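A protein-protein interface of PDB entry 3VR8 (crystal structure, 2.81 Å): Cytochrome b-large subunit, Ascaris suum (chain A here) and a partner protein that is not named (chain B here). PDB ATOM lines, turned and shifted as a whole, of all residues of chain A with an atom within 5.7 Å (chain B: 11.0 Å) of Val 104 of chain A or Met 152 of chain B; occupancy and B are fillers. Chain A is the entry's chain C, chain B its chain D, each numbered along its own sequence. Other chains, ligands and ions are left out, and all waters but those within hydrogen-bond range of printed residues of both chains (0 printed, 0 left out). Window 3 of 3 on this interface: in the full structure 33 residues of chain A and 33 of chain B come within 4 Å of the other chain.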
ATOM      1  N   ASP A  99      17.146 -26.235 -15.664  1.00  0.00           N
ATOM      2  CA  ASP A  99      16.201 -27.238 -15.126  1.00  0.00           C
ATOM      3  C   ASP A  99      14.724 -26.954 -15.512  1.00  0.00           C
ATOM      4  O   ASP A  99      14.454 -25.968 -16.210  1.00  0.00           O
ATOM      5  CB  ASP A  99      16.400 -27.417 -13.614  1.00  0.00           C
ATOM      6  CG  ASP A  99      15.491 -26.521 -12.777  1.00  0.00           C
ATOM      7  OD1 ASP A  99      14.317 -26.897 -12.553  1.00  0.00           O
ATOM      8  OD2 ASP A  99      15.954 -25.452 -12.319  1.00  0.00           O
ATOM      9  N   PHE A 100      13.791 -27.807 -15.066  1.00  0.00           N
ATOM     10  CA  PHE A 100      12.361 -27.749 -15.472  1.00  0.00           C
ATOM     11  C   PHE A 100      11.597 -26.508 -14.998  1.00  0.00           C
ATOM     12  O   PHE A 100      10.803 -25.950 -15.751  1.00  0.00           O
ATOM     13  CB  PHE A 100      11.613 -29.028 -15.041  1.00  0.00           C
ATOM     14  CG  PHE A 100      10.224 -29.184 -15.645  1.00  0.00           C
ATOM     15  CD1 PHE A 100       9.085 -29.013 -14.868  1.00  0.00           C
ATOM     16  CD2 PHE A 100      10.051 -29.530 -16.980  1.00  0.00           C
ATOM     17  CE1 PHE A 100       7.805 -29.167 -15.415  1.00  0.00           C
ATOM     18  CE2 PHE A 100       8.761 -29.678 -17.522  1.00  0.00           C
ATOM     19  CZ  PHE A 100       7.650 -29.503 -16.731  1.00  0.00           C
ATOM     20  N   THR A 101      11.836 -26.091 -13.755  1.00  0.00           N
ATOM     21  CA  THR A 101      11.177 -24.917 -13.168  1.00  0.00           C
ATOM     22  C   THR A 101      11.563 -23.652 -13.931  1.00  0.00           C
ATOM     23  O   THR A 101      10.705 -22.847 -14.284  1.00  0.00           O
ATOM     24  CB  THR A 101      11.502 -24.777 -11.652  1.00  0.00           C
ATOM     25  OG1 THR A 101      11.205 -26.007 -10.978  1.00  0.00           O
ATOM     26  CG2 THR A 101      10.685 -23.681 -11.014  1.00  0.00           C
ATOM     27  N   THR A 102      12.854 -23.496 -14.206  1.00  0.00           N
ATOM     28  CA  THR A 102      13.355 -22.334 -14.953  1.00  0.00           C
ATOM     29  C   THR A 102      12.931 -22.370 -16.439  1.00  0.00           C
ATOM     30  O   THR A 102      12.900 -21.335 -17.104  1.00  0.00           O
ATOM     31  CB  THR A 102      14.900 -22.161 -14.781  1.00  0.00           C
ATOM     32  OG1 THR A 102      15.590 -23.244 -15.411  1.00  0.00           O
ATOM     33  CG2 THR A 102      15.287 -22.143 -13.304  1.00  0.00           C
ATOM     34  N   PHE A 103      12.587 -23.570 -16.923  1.00  0.00           N
ATOM     35  CA  PHE A 103      12.166 -23.828 -18.311  1.00  0.00           C
ATOM     36  C   PHE A 103      10.646 -23.680 -18.469  1.00  0.00           C
ATOM     37  O   PHE A 103      10.167 -23.176 -19.483  1.00  0.00           O
ATOM     38  CB  PHE A 103      12.670 -25.219 -18.760  1.00  0.00           C
ATOM     39  CG  PHE A 103      11.987 -25.785 -20.001  1.00  0.00           C
ATOM     40  CD1 PHE A 103      12.531 -25.583 -21.271  1.00  0.00           C
ATOM     41  CD2 PHE A 103      10.822 -26.564 -19.892  1.00  0.00           C
ATOM     42  CE1 PHE A 103      11.904 -26.118 -22.412  1.00  0.00           C
ATOM     43  CE2 PHE A 103      10.193 -27.105 -21.036  1.00  0.00           C
ATOM     44  CZ  PHE A 103      10.737 -26.878 -22.292  1.00  0.00           C
ATOM     45  N   VAL A 104       9.893 -24.108 -17.463  1.00  0.00           N
ATOM     46  CA  VAL A 104       8.439 -23.905 -17.451  1.00  0.00           C
ATOM     47  C   VAL A 104       8.052 -22.424 -17.547  1.00  0.00           C
ATOM     48  O   VAL A 104       6.904 -22.093 -17.858  1.00  0.00           O
ATOM     49  CB  VAL A 104       7.768 -24.613 -16.236  1.00  0.00           C
ATOM     50  CG1 VAL A 104       6.555 -23.843 -15.698  1.00  0.00           C
ATOM     51  CG2 VAL A 104       7.383 -26.015 -16.623  1.00  0.00           C
ATOM     52  N   GLU A 105       9.009 -21.532 -17.301  1.00  0.00           N
ATOM     53  CA  GLU A 105       8.761 -20.122 -17.573  1.00  0.00           C
ATOM     54  C   GLU A 105       9.785 -19.407 -18.481  1.00  0.00           C
ATOM     55  O   GLU A 105       9.685 -18.193 -18.707  1.00  0.00           O
ATOM     56  CB  GLU A 105       8.392 -19.349 -16.293  1.00  0.00           C
ATOM     57  CG  GLU A 105       9.507 -19.040 -15.325  1.00  0.00           C
ATOM     58  CD  GLU A 105       9.167 -17.833 -14.451  1.00  0.00           C
ATOM     59  OE1 GLU A 105       9.090 -17.999 -13.212  1.00  0.00           O
ATOM     60  OE2 GLU A 105       8.955 -16.721 -15.001  1.00  0.00           O
ATOM     61  N   PHE A 106      10.739 -20.165 -19.029  1.00  0.00           N
ATOM     62  CA  PHE A 106      11.560 -19.706 -20.164  1.00  0.00           C
ATOM     63  C   PHE A 106      10.647 -19.750 -21.386  1.00  0.00           C
ATOM     64  O   PHE A 106      11.070 -19.431 -22.507  1.00  0.00           O
ATOM     65  CB  PHE A 106      12.758 -20.645 -20.383  1.00  0.00           C
ATOM     66  CG  PHE A 106      14.054 -19.950 -20.813  1.00  0.00           C
ATOM     67  CD1 PHE A 106      15.087 -19.722 -19.877  1.00  0.00           C
ATOM     68  CD2 PHE A 106      14.266 -19.576 -22.154  1.00  0.00           C
ATOM     69  CE1 PHE A 106      16.301 -19.104 -20.256  1.00  0.00           C
ATOM     70  CE2 PHE A 106      15.483 -18.953 -22.549  1.00  0.00           C
ATOM     71  CZ  PHE A 106      16.500 -18.716 -21.594  1.00  0.00           C
ATOM     72  N   ILE A 107       9.401 -20.180 -21.142  1.00  0.00           N
ATOM     73  CA  ILE A 107       8.349 -20.296 -22.163  1.00  0.00           C
ATOM     74  C   ILE A 107       7.038 -19.566 -21.784  1.00  0.00           C
ATOM     75  O   ILE A 107       6.308 -19.107 -22.674  1.00  0.00           O
ATOM     76  CB  ILE A 107       8.089 -21.792 -22.624  1.00  0.00           C
ATOM     77  CG1 ILE A 107       7.157 -22.543 -21.681  1.00  0.00           C
ATOM     78  CG2 ILE A 107       9.391 -22.567 -22.838  1.00  0.00           C
ATOM     79  CD1 ILE A 107       5.792 -22.738 -22.260  1.00  0.00           C
ATOM     80  N   ARG A 108       6.737 -19.468 -20.485  1.00  0.00           N
ATOM     81  CA  ARG A 108       5.634 -18.618 -20.014  1.00  0.00           C
ATOM     82  C   ARG A 108       5.947 -17.148 -20.290  1.00  0.00           C
ATOM     83  O   ARG A 108       5.050 -16.355 -20.583  1.00  0.00           O
ATOM     84  CB  ARG A 108       5.337 -18.829 -18.520  1.00  0.00           C
ATOM     85  CG  ARG A 108       4.392 -17.765 -17.895  1.00  0.00           C
ATOM     86  CD  ARG A 108       3.798 -18.165 -16.532  1.00  0.00           C
ATOM     87  NE  ARG A 108       4.825 -18.453 -15.523  1.00  0.00           N
ATOM     88  CZ  ARG A 108       4.853 -19.536 -14.738  1.00  0.00           C
ATOM     89  NH1 ARG A 108       3.892 -20.459 -14.810  1.00  0.00           N
ATOM     90  NH2 ARG A 108       5.846 -19.691 -13.865  1.00  0.00           N
ATOM     91  N   HIS B  80      -1.522 -37.123  -6.554  1.00  0.00           N
ATOM     92  CA  HIS B  80      -0.186 -36.733  -6.974  1.00  0.00           C
ATOM     93  C   HIS B  80       0.897 -36.873  -5.882  1.00  0.00           C
ATOM     94  O   HIS B  80       0.776 -37.697  -4.961  1.00  0.00           O
ATOM     95  CB  HIS B  80      -0.234 -35.301  -7.444  1.00  0.00           C
ATOM     96  CG  HIS B  80      -0.795 -35.144  -8.810  1.00  0.00           C
ATOM     97  ND1 HIS B  80      -0.578 -34.017  -9.573  1.00  0.00           N
ATOM     98  CD2 HIS B  80      -1.546 -35.979  -9.565  1.00  0.00           C
ATOM     99  CE1 HIS B  80      -1.192 -34.155 -10.737  1.00  0.00           C
ATOM    100  NE2 HIS B  80      -1.783 -35.339 -10.759  1.00  0.00           N
ATOM    101  N   ARG B  82       4.969 -37.295  -4.238  1.00  0.00           N
ATOM    102  CA  ARG B  82       6.311 -37.861  -4.397  1.00  0.00           C
ATOM    103  C   ARG B  82       6.336 -39.389  -4.470  1.00  0.00           C
ATOM    104  O   ARG B  82       7.300 -39.967  -4.960  1.00  0.00           O
ATOM    105  CB  ARG B  82       7.248 -37.330  -3.294  1.00  0.00           C
ATOM    106  CG  ARG B  82       8.762 -37.455  -3.550  1.00  0.00           C
ATOM    107  CD  ARG B  82       9.371 -36.328  -4.421  1.00  0.00           C
ATOM    108  NE  ARG B  82       9.501 -35.034  -3.728  1.00  0.00           N
ATOM    109  CZ  ARG B  82       9.653 -33.849  -4.338  1.00  0.00           C
ATOM    110  NH1 ARG B  82       9.708 -33.762  -5.667  1.00  0.00           N
ATOM    111  NH2 ARG B  82       9.756 -32.732  -3.618  1.00  0.00           N
ATOM    112  N   ASP B  85       4.904 -40.434  -8.288  1.00  0.00           N
ATOM    113  CA  ASP B  85       6.094 -40.100  -9.079  1.00  0.00           C
ATOM    114  C   ASP B  85       7.087 -41.265  -9.173  1.00  0.00           C
ATOM    115  O   ASP B  85       7.627 -41.531 -10.236  1.00  0.00           O
ATOM    116  CB  ASP B  85       6.799 -38.856  -8.499  1.00  0.00           C
ATOM    117  CG  ASP B  85       6.268 -37.512  -9.074  1.00  0.00           C
ATOM    118  OD1 ASP B  85       6.708 -36.437  -8.589  1.00  0.00           O
ATOM    119  OD2 ASP B  85       5.434 -37.514 -10.011  1.00  0.00           O
ATOM    120  N   PHE B 139      15.170 -37.084 -12.012  1.00  0.00           N
ATOM    121  CA  PHE B 139      14.112 -36.056 -12.101  1.00  0.00           C
ATOM    122  C   PHE B 139      13.139 -36.061 -10.911  1.00  0.00           C
ATOM    123  O   PHE B 139      12.655 -35.010 -10.489  1.00  0.00           O
ATOM    124  CB  PHE B 139      13.327 -36.254 -13.406  1.00  0.00           C
ATOM    125  CG  PHE B 139      12.442 -35.094 -13.794  1.00  0.00           C
ATOM    126  CD1 PHE B 139      12.942 -34.044 -14.557  1.00  0.00           C
ATOM    127  CD2 PHE B 139      11.095 -35.076 -13.440  1.00  0.00           C
ATOM    128  CE1 PHE B 139      12.127 -32.980 -14.940  1.00  0.00           C
ATOM    129  CE2 PHE B 139      10.275 -34.018 -13.820  1.00  0.00           C
ATOM    130  CZ  PHE B 139      10.795 -32.968 -14.569  1.00  0.00           C
ATOM    131  N   HIS B 142      15.566 -34.762  -7.917  1.00  0.00           N
ATOM    132  CA  HIS B 142      16.176 -33.436  -7.903  1.00  0.00           C
ATOM    133  C   HIS B 142      15.344 -32.350  -8.491  1.00  0.00           C
ATOM    134  O   HIS B 142      15.334 -31.242  -7.971  1.00  0.00           O
ATOM    135  CB  HIS B 142      17.587 -33.463  -8.461  1.00  0.00           C
ATOM    136  CG  HIS B 142      18.513 -34.243  -7.592  1.00  0.00           C
ATOM    137  ND1 HIS B 142      18.696 -35.600  -7.738  1.00  0.00           N
ATOM    138  CD2 HIS B 142      19.216 -33.883  -6.493  1.00  0.00           C
ATOM    139  CE1 HIS B 142      19.516 -36.037  -6.799  1.00  0.00           C
ATOM    140  NE2 HIS B 142      19.847 -35.015  -6.030  1.00  0.00           N
ATOM    141  N   ASP B 143      14.610 -32.653  -9.547  1.00  0.00           N
ATOM    142  CA  ASP B 143      13.640 -31.680 -10.021  1.00  0.00           C
ATOM    143  C   ASP B 143      12.250 -31.922  -9.414  1.00  0.00           C
ATOM    144  O   ASP B 143      12.107 -32.666  -8.430  1.00  0.00           O
ATOM    145  CB  ASP B 143      13.611 -31.618 -11.546  1.00  0.00           C
ATOM    146  CG  ASP B 143      13.448 -30.198 -12.058  1.00  0.00           C
ATOM    147  OD1 ASP B 143      14.204 -29.822 -12.987  1.00  0.00           O
ATOM    148  OD2 ASP B 143      12.577 -29.454 -11.524  1.00  0.00           O
ATOM    149  N   VAL B 144      11.236 -31.304 -10.006  1.00  0.00           N
ATOM    150  CA  VAL B 144       9.907 -31.253  -9.426  1.00  0.00           C
ATOM    151  C   VAL B 144       9.123 -32.578  -9.356  1.00  0.00           C
ATOM    152  O   VAL B 144       8.105 -32.666  -8.674  1.00  0.00           O
ATOM    153  CB  VAL B 144       9.091 -30.192 -10.137  1.00  0.00           C
ATOM    154  CG1 VAL B 144       9.262 -28.850  -9.438  1.00  0.00           C
ATOM    155  CG2 VAL B 144       9.525 -30.098 -11.582  1.00  0.00           C
ATOM    156  N   GLY B 145       9.609 -33.612 -10.038  1.00  0.00           N
ATOM    157  CA  GLY B 145       8.903 -34.896 -10.117  1.00  0.00           C
ATOM    158  C   GLY B 145       7.979 -34.922 -11.324  1.00  0.00           C
ATOM    159  O   GLY B 145       7.613 -33.865 -11.848  1.00  0.00           O
ATOM    160  N   LEU B 146       7.606 -36.117 -11.781  1.00  0.00           N
ATOM    161  CA  LEU B 146       6.708 -36.236 -12.932  1.00  0.00           C
ATOM    162  C   LEU B 146       5.420 -35.491 -12.699  1.00  0.00           C
ATOM    163  O   LEU B 146       5.036 -34.667 -13.521  1.00  0.00           O
ATOM    164  CB  LEU B 146       6.401 -37.690 -13.287  1.00  0.00           C
ATOM    165  CG  LEU B 146       7.545 -38.467 -13.928  1.00  0.00           C
ATOM    166  CD1 LEU B 146       7.214 -39.955 -13.981  1.00  0.00           C
ATOM    167  CD2 LEU B 146       7.885 -37.903 -15.319  1.00  0.00           C
ATOM    168  N   THR B 147       4.763 -35.753 -11.576  1.00  0.00           N
ATOM    169  CA  THR B 147       3.438 -35.217 -11.382  1.00  0.00           C
ATOM    170  C   THR B 147       3.425 -33.705 -11.231  1.00  0.00           C
ATOM    171  O   THR B 147       2.543 -33.066 -11.790  1.00  0.00           O
ATOM    172  CB  THR B 147       2.685 -35.883 -10.236  1.00  0.00           C
ATOM    173  OG1 THR B 147       3.494 -35.854  -9.061  1.00  0.00           O
ATOM    174  CG2 THR B 147       2.354 -37.321 -10.583  1.00  0.00           C
ATOM    175  N   ARG B 148       4.387 -33.119 -10.516  1.00  0.00           N
ATOM    176  CA  ARG B 148       4.437 -31.651 -10.427  1.00  0.00           C
ATOM    177  C   ARG B 148       4.792 -31.056 -11.795  1.00  0.00           C
ATOM    178  O   ARG B 148       4.269 -30.005 -12.193  1.00  0.00           O
ATOM    179  CB  ARG B 148       5.395 -31.159  -9.335  1.00  0.00           C
ATOM    180  CG  ARG B 148       5.130 -29.683  -8.835  1.00  0.00           C
ATOM    181  CD  ARG B 148       6.049 -29.286  -7.613  1.00  0.00           C
ATOM    182  NE  ARG B 148       6.245 -30.406  -6.653  1.00  0.00           N
ATOM    183  CZ  ARG B 148       7.152 -30.463  -5.666  1.00  0.00           C
ATOM    184  NH1 ARG B 148       7.989 -29.450  -5.452  1.00  0.00           N
ATOM    185  NH2 ARG B 148       7.217 -31.549  -4.887  1.00  0.00           N
ATOM    186  N   ALA B 149       5.667 -31.751 -12.517  1.00  0.00           N
ATOM    187  CA  ALA B 149       6.007 -31.383 -13.882  1.00  0.00           C
ATOM    188  C   ALA B 149       4.749 -31.229 -14.729  1.00  0.00           C
ATOM    189  O   ALA B 149       4.575 -30.203 -15.390  1.00  0.00           O
ATOM    190  CB  ALA B 149       6.960 -32.402 -14.490  1.00  0.00           C
ATOM    191  N   PHE B 150       3.875 -32.238 -14.688  1.00  0.00           N
ATOM    192  CA  PHE B 150       2.549 -32.162 -15.314  1.00  0.00           C
ATOM    193  C   PHE B 150       1.770 -30.915 -14.901  1.00  0.00           C
ATOM    194  O   PHE B 150       1.281 -30.174 -15.758  1.00  0.00           O
ATOM    195  CB  PHE B 150       1.718 -33.421 -15.030  1.00  0.00           C
ATOM    196  CG  PHE B 150       1.844 -34.479 -16.088  1.00  0.00           C
ATOM    197  CD1 PHE B 150       2.478 -35.670 -15.821  1.00  0.00           C
ATOM    198  CD2 PHE B 150       1.337 -34.275 -17.360  1.00  0.00           C
ATOM    199  CE1 PHE B 150       2.601 -36.634 -16.797  1.00  0.00           C
ATOM    200  CE2 PHE B 150       1.464 -35.238 -18.333  1.00  0.00           C
ATOM    201  CZ  PHE B 150       2.094 -36.414 -18.049  1.00  0.00           C
ATOM    202  N   GLU B 151       1.676 -30.683 -13.591  1.00  0.00           N
ATOM    203  CA  GLU B 151       0.951 -29.530 -13.052  1.00  0.00           C
ATOM    204  C   GLU B 151       1.455 -28.255 -13.690  1.00  0.00           C
ATOM    205  O   GLU B 151       0.674 -27.496 -14.248  1.00  0.00           O
ATOM    206  CB  GLU B 151       1.079 -29.423 -11.522  1.00  0.00           C
ATOM    207  CG  GLU B 151       0.383 -30.523 -10.714  1.00  0.00           C
ATOM    208  CD  GLU B 151       0.649 -30.431  -9.212  1.00  0.00           C
ATOM    209  OE1 GLU B 151       0.794 -31.499  -8.557  1.00  0.00           O
ATOM    210  OE2 GLU B 151       0.715 -29.297  -8.687  1.00  0.00           O
ATOM    211  N   MET B 152       2.764 -28.048 -13.631  1.00  0.00           N
ATOM    212  CA  MET B 152       3.355 -26.760 -14.007  1.00  0.00           C
ATOM    213  C   MET B 152       3.206 -26.372 -15.479  1.00  0.00           C
ATOM    214  O   MET B 152       3.064 -25.182 -15.795  1.00  0.00           O
ATOM    215  CB  MET B 152       4.813 -26.695 -13.577  1.00  0.00           C
ATOM    216  CG  MET B 152       4.978 -26.513 -12.083  1.00  0.00           C
ATOM    217  SD  MET B 152       6.426 -27.385 -11.489  1.00  0.00           S
ATOM    218  CE  MET B 152       7.744 -26.585 -12.431  1.00  0.00           C
ATOM    219  N   VAL B 153       3.237 -27.376 -16.360  1.00  0.00           N
ATOM    220  CA  VAL B 153       2.962 -27.161 -17.778  1.00  0.00           C
ATOM    221  C   VAL B 153       1.471 -26.916 -17.983  1.00  0.00           C
ATOM    222  O   VAL B 153       1.087 -26.128 -18.842  1.00  0.00           O
ATOM    223  CB  VAL B 153       3.458 -28.323 -18.682  1.00  0.00           C
ATOM    224  CG1 VAL B 153       4.882 -28.657 -18.368  1.00  0.00           C
ATOM    225  CG2 VAL B 153       2.602 -29.559 -18.529  1.00  0.00           C
ATOM    226  N   TRP B 154       0.641 -27.580 -17.179  1.00  0.00           N
ATOM    227  CA  TRP B 154      -0.807 -27.388 -17.238  1.00  0.00           C
ATOM    228  C   TRP B 154      -1.291 -26.074 -16.601  1.00  0.00           C
ATOM    229  O   TRP B 154      -2.460 -25.697 -16.736  1.00  0.00           O
ATOM    230  CB  TRP B 154      -1.530 -28.590 -16.639  1.00  0.00           C
ATOM    231  CG  TRP B 154      -2.390 -29.321 -17.620  1.00  0.00           C
ATOM    232  CD1 TRP B 154      -3.720 -29.121 -17.843  1.00  0.00           C
ATOM    233  CD2 TRP B 154      -1.987 -30.374 -18.513  1.00  0.00           C
ATOM    234  NE1 TRP B 154      -4.173 -29.984 -18.813  1.00  0.00           N
ATOM    235  CE2 TRP B 154      -3.130 -30.761 -19.245  1.00  0.00           C
ATOM    236  CE3 TRP B 154      -0.774 -31.032 -18.763  1.00  0.00           C
ATOM    237  CZ2 TRP B 154      -3.095 -31.774 -20.208  1.00  0.00           C
ATOM    238  CZ3 TRP B 154      -0.746 -32.039 -19.726  1.00  0.00           C
ATOM    239  CH2 TRP B 154      -1.894 -32.393 -20.434  1.00  0.00           C
ATOM    240  N   GLU B 155      -0.387 -25.367 -15.932  1.00  0.00           N
ATOM    241  CA  GLU B 155      -0.739 -24.104 -15.284  1.00  0.00           C
ATOM    242  C   GLU B 155      -0.677 -22.903 -16.232  1.00  0.00           C
ATOM    243  O   GLU B 155      -1.227 -21.844 -15.924  1.00  0.00           O
ATOM    244  CB  GLU B 155       0.126 -23.868 -14.025  1.00  0.00           C
ATOM    245  CG  GLU B 155      -0.291 -24.751 -12.807  1.00  0.00           C
ATOM    246  CD  GLU B 155       0.302 -24.300 -11.464  1.00  0.00           C
ATOM    247  OE1 GLU B 155       1.293 -23.544 -11.457  1.00  0.00           O
ATOM    248  OE2 GLU B 155      -0.230 -24.704 -10.406  1.00  0.00           O
ATOM    249  N   LEU B 156      -0.021 -23.080 -17.381  1.00  0.00           N
ATOM    250  CA  LEU B 156       0.239 -21.970 -18.315  1.00  0.00           C
ATOM    251  C   LEU B 156      -0.740 -21.909 -19.478  1.00  0.00           C
ATOM    252  O   LEU B 156      -1.343 -20.861 -19.727  1.00  0.00           O
ATOM    253  CB  LEU B 156       1.699 -21.949 -18.826  1.00  0.00           C
ATOM    254  CG  LEU B 156       2.661 -23.145 -19.001  1.00  0.00           C
ATOM    255  CD1 LEU B 156       2.333 -24.054 -20.161  1.00  0.00           C
ATOM    256  CD2 LEU B 156       4.050 -22.605 -19.200  1.00  0.00           C
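Val 104 of chain A touches just these residues of chain B: Met 152 and Leu 156.
Phe 100 of chain A touches six residues of chain B.
No residue of chain B comes within 4 Å of Phe 103 of chain A.
No residue of chain B comes within 4 Å of Glu 105 of chain A.
Of chain B, only Leu 156 (3.5 Å) comes within 4 Å of Ile 107 of chain A.
No residue of chain B comes within 4 Å of Arg 108 of chain A.
Of the printed residues of chain A, Val 153 of chain B touches Phe 100.
Printed residues of chain A within 4 Å of Val 144 of chain B: Phe 100 (3.5 Å) and Thr 101 (3.8 Å).
Of the printed residues of chain A, Ala 149 of chain B touches Phe 100 (3.2 Å).
Of the printed residues of chain B, Asp 99 of chain A touches Asp 143 (3.0 Å).
Of the printed residues of chain A, Asp 143 of chain B touches Asp 99, Phe 100 and Thr 101.
The nearest residue of chain A that does not touch Met 152 of chain B is Arg 108 of chain A (4.9 Å).
The backbone NH (N) of Phe 100 of chain A sits at hydrogen-bond distance from the side-chain carboxylate (OD1) of Asp 143 of chain B.
The side-chain carboxylate (OD1) of Asp 143 of chain B sits close to the side-chain carboxylate (OD1) of Asp 99 of chain A.
OD1 of Asp 99 of chain A lies within hydrogen-bond range of N of Thr 101 of chain A (2.9 Å).
The side-chain hydroxyl (OG1) of Thr 102 of chain A lies within hydrogen-bond range of the backbone carbonyl oxygen (O) of Asp 99 of chain A (3.1 Å).
The backbone NH of Gly 145 of chain B is in hydrogen-bond range of the backbone carbonyl oxygen of Phe 139 of chain B, at 3.4 Å.
Phe 100 of chain A touches Phe 139 of chain B (CG to CZ, 3.98 Å).
CD1 of Phe 100 of chain A touches CG2 of Val 144 of chain B, 3.5 Å away.
Ala 149 of chain B touches Phe 100 of chain A (CA to CE1, 3.2 Å).
CD1 of Phe 100 of chain A touches CE of Met 152 of chain B (3.7 Å).
CZ of Phe 100 of chain A touches CG1 of Val 153 of chain B, 3.3 Å away.
OG1 of Thr 101 of chain A touches OD2 of Asp 143 of chain B, at 3.7 Å.
OG1 of Thr 101 of chain A touches CG1 of Val 144 of chain B, at 3.8 Å.
Thr 101 of chain A touches Met 152 of chain B (OG1 to CE, 3.8 Å).
Val 104 of chain A touches Leu 156 of chain B (O to CD2, 3.2 Å).
Leu 156 of chain B touches Ile 107 of chain A (CD2 to CD1, 3.5 Å).
Of the 10 printed residues of chain A, 5 touch a printed residue of chain B.
Printed residues of chain A that touch a printed residue of chain B: Asp 99, Phe 100, Thr 101, Val 104 and Ile 107.
Of the 19 printed residues of chain B, 7 touch a printed residue of chain A.
Among the printed residues, 13 pairs touch across the chains.
Among the printed residues, no Asp or Glu carboxylate lies within 4 Å of a Lys or Arg side-chain nitrogen of the other chain.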
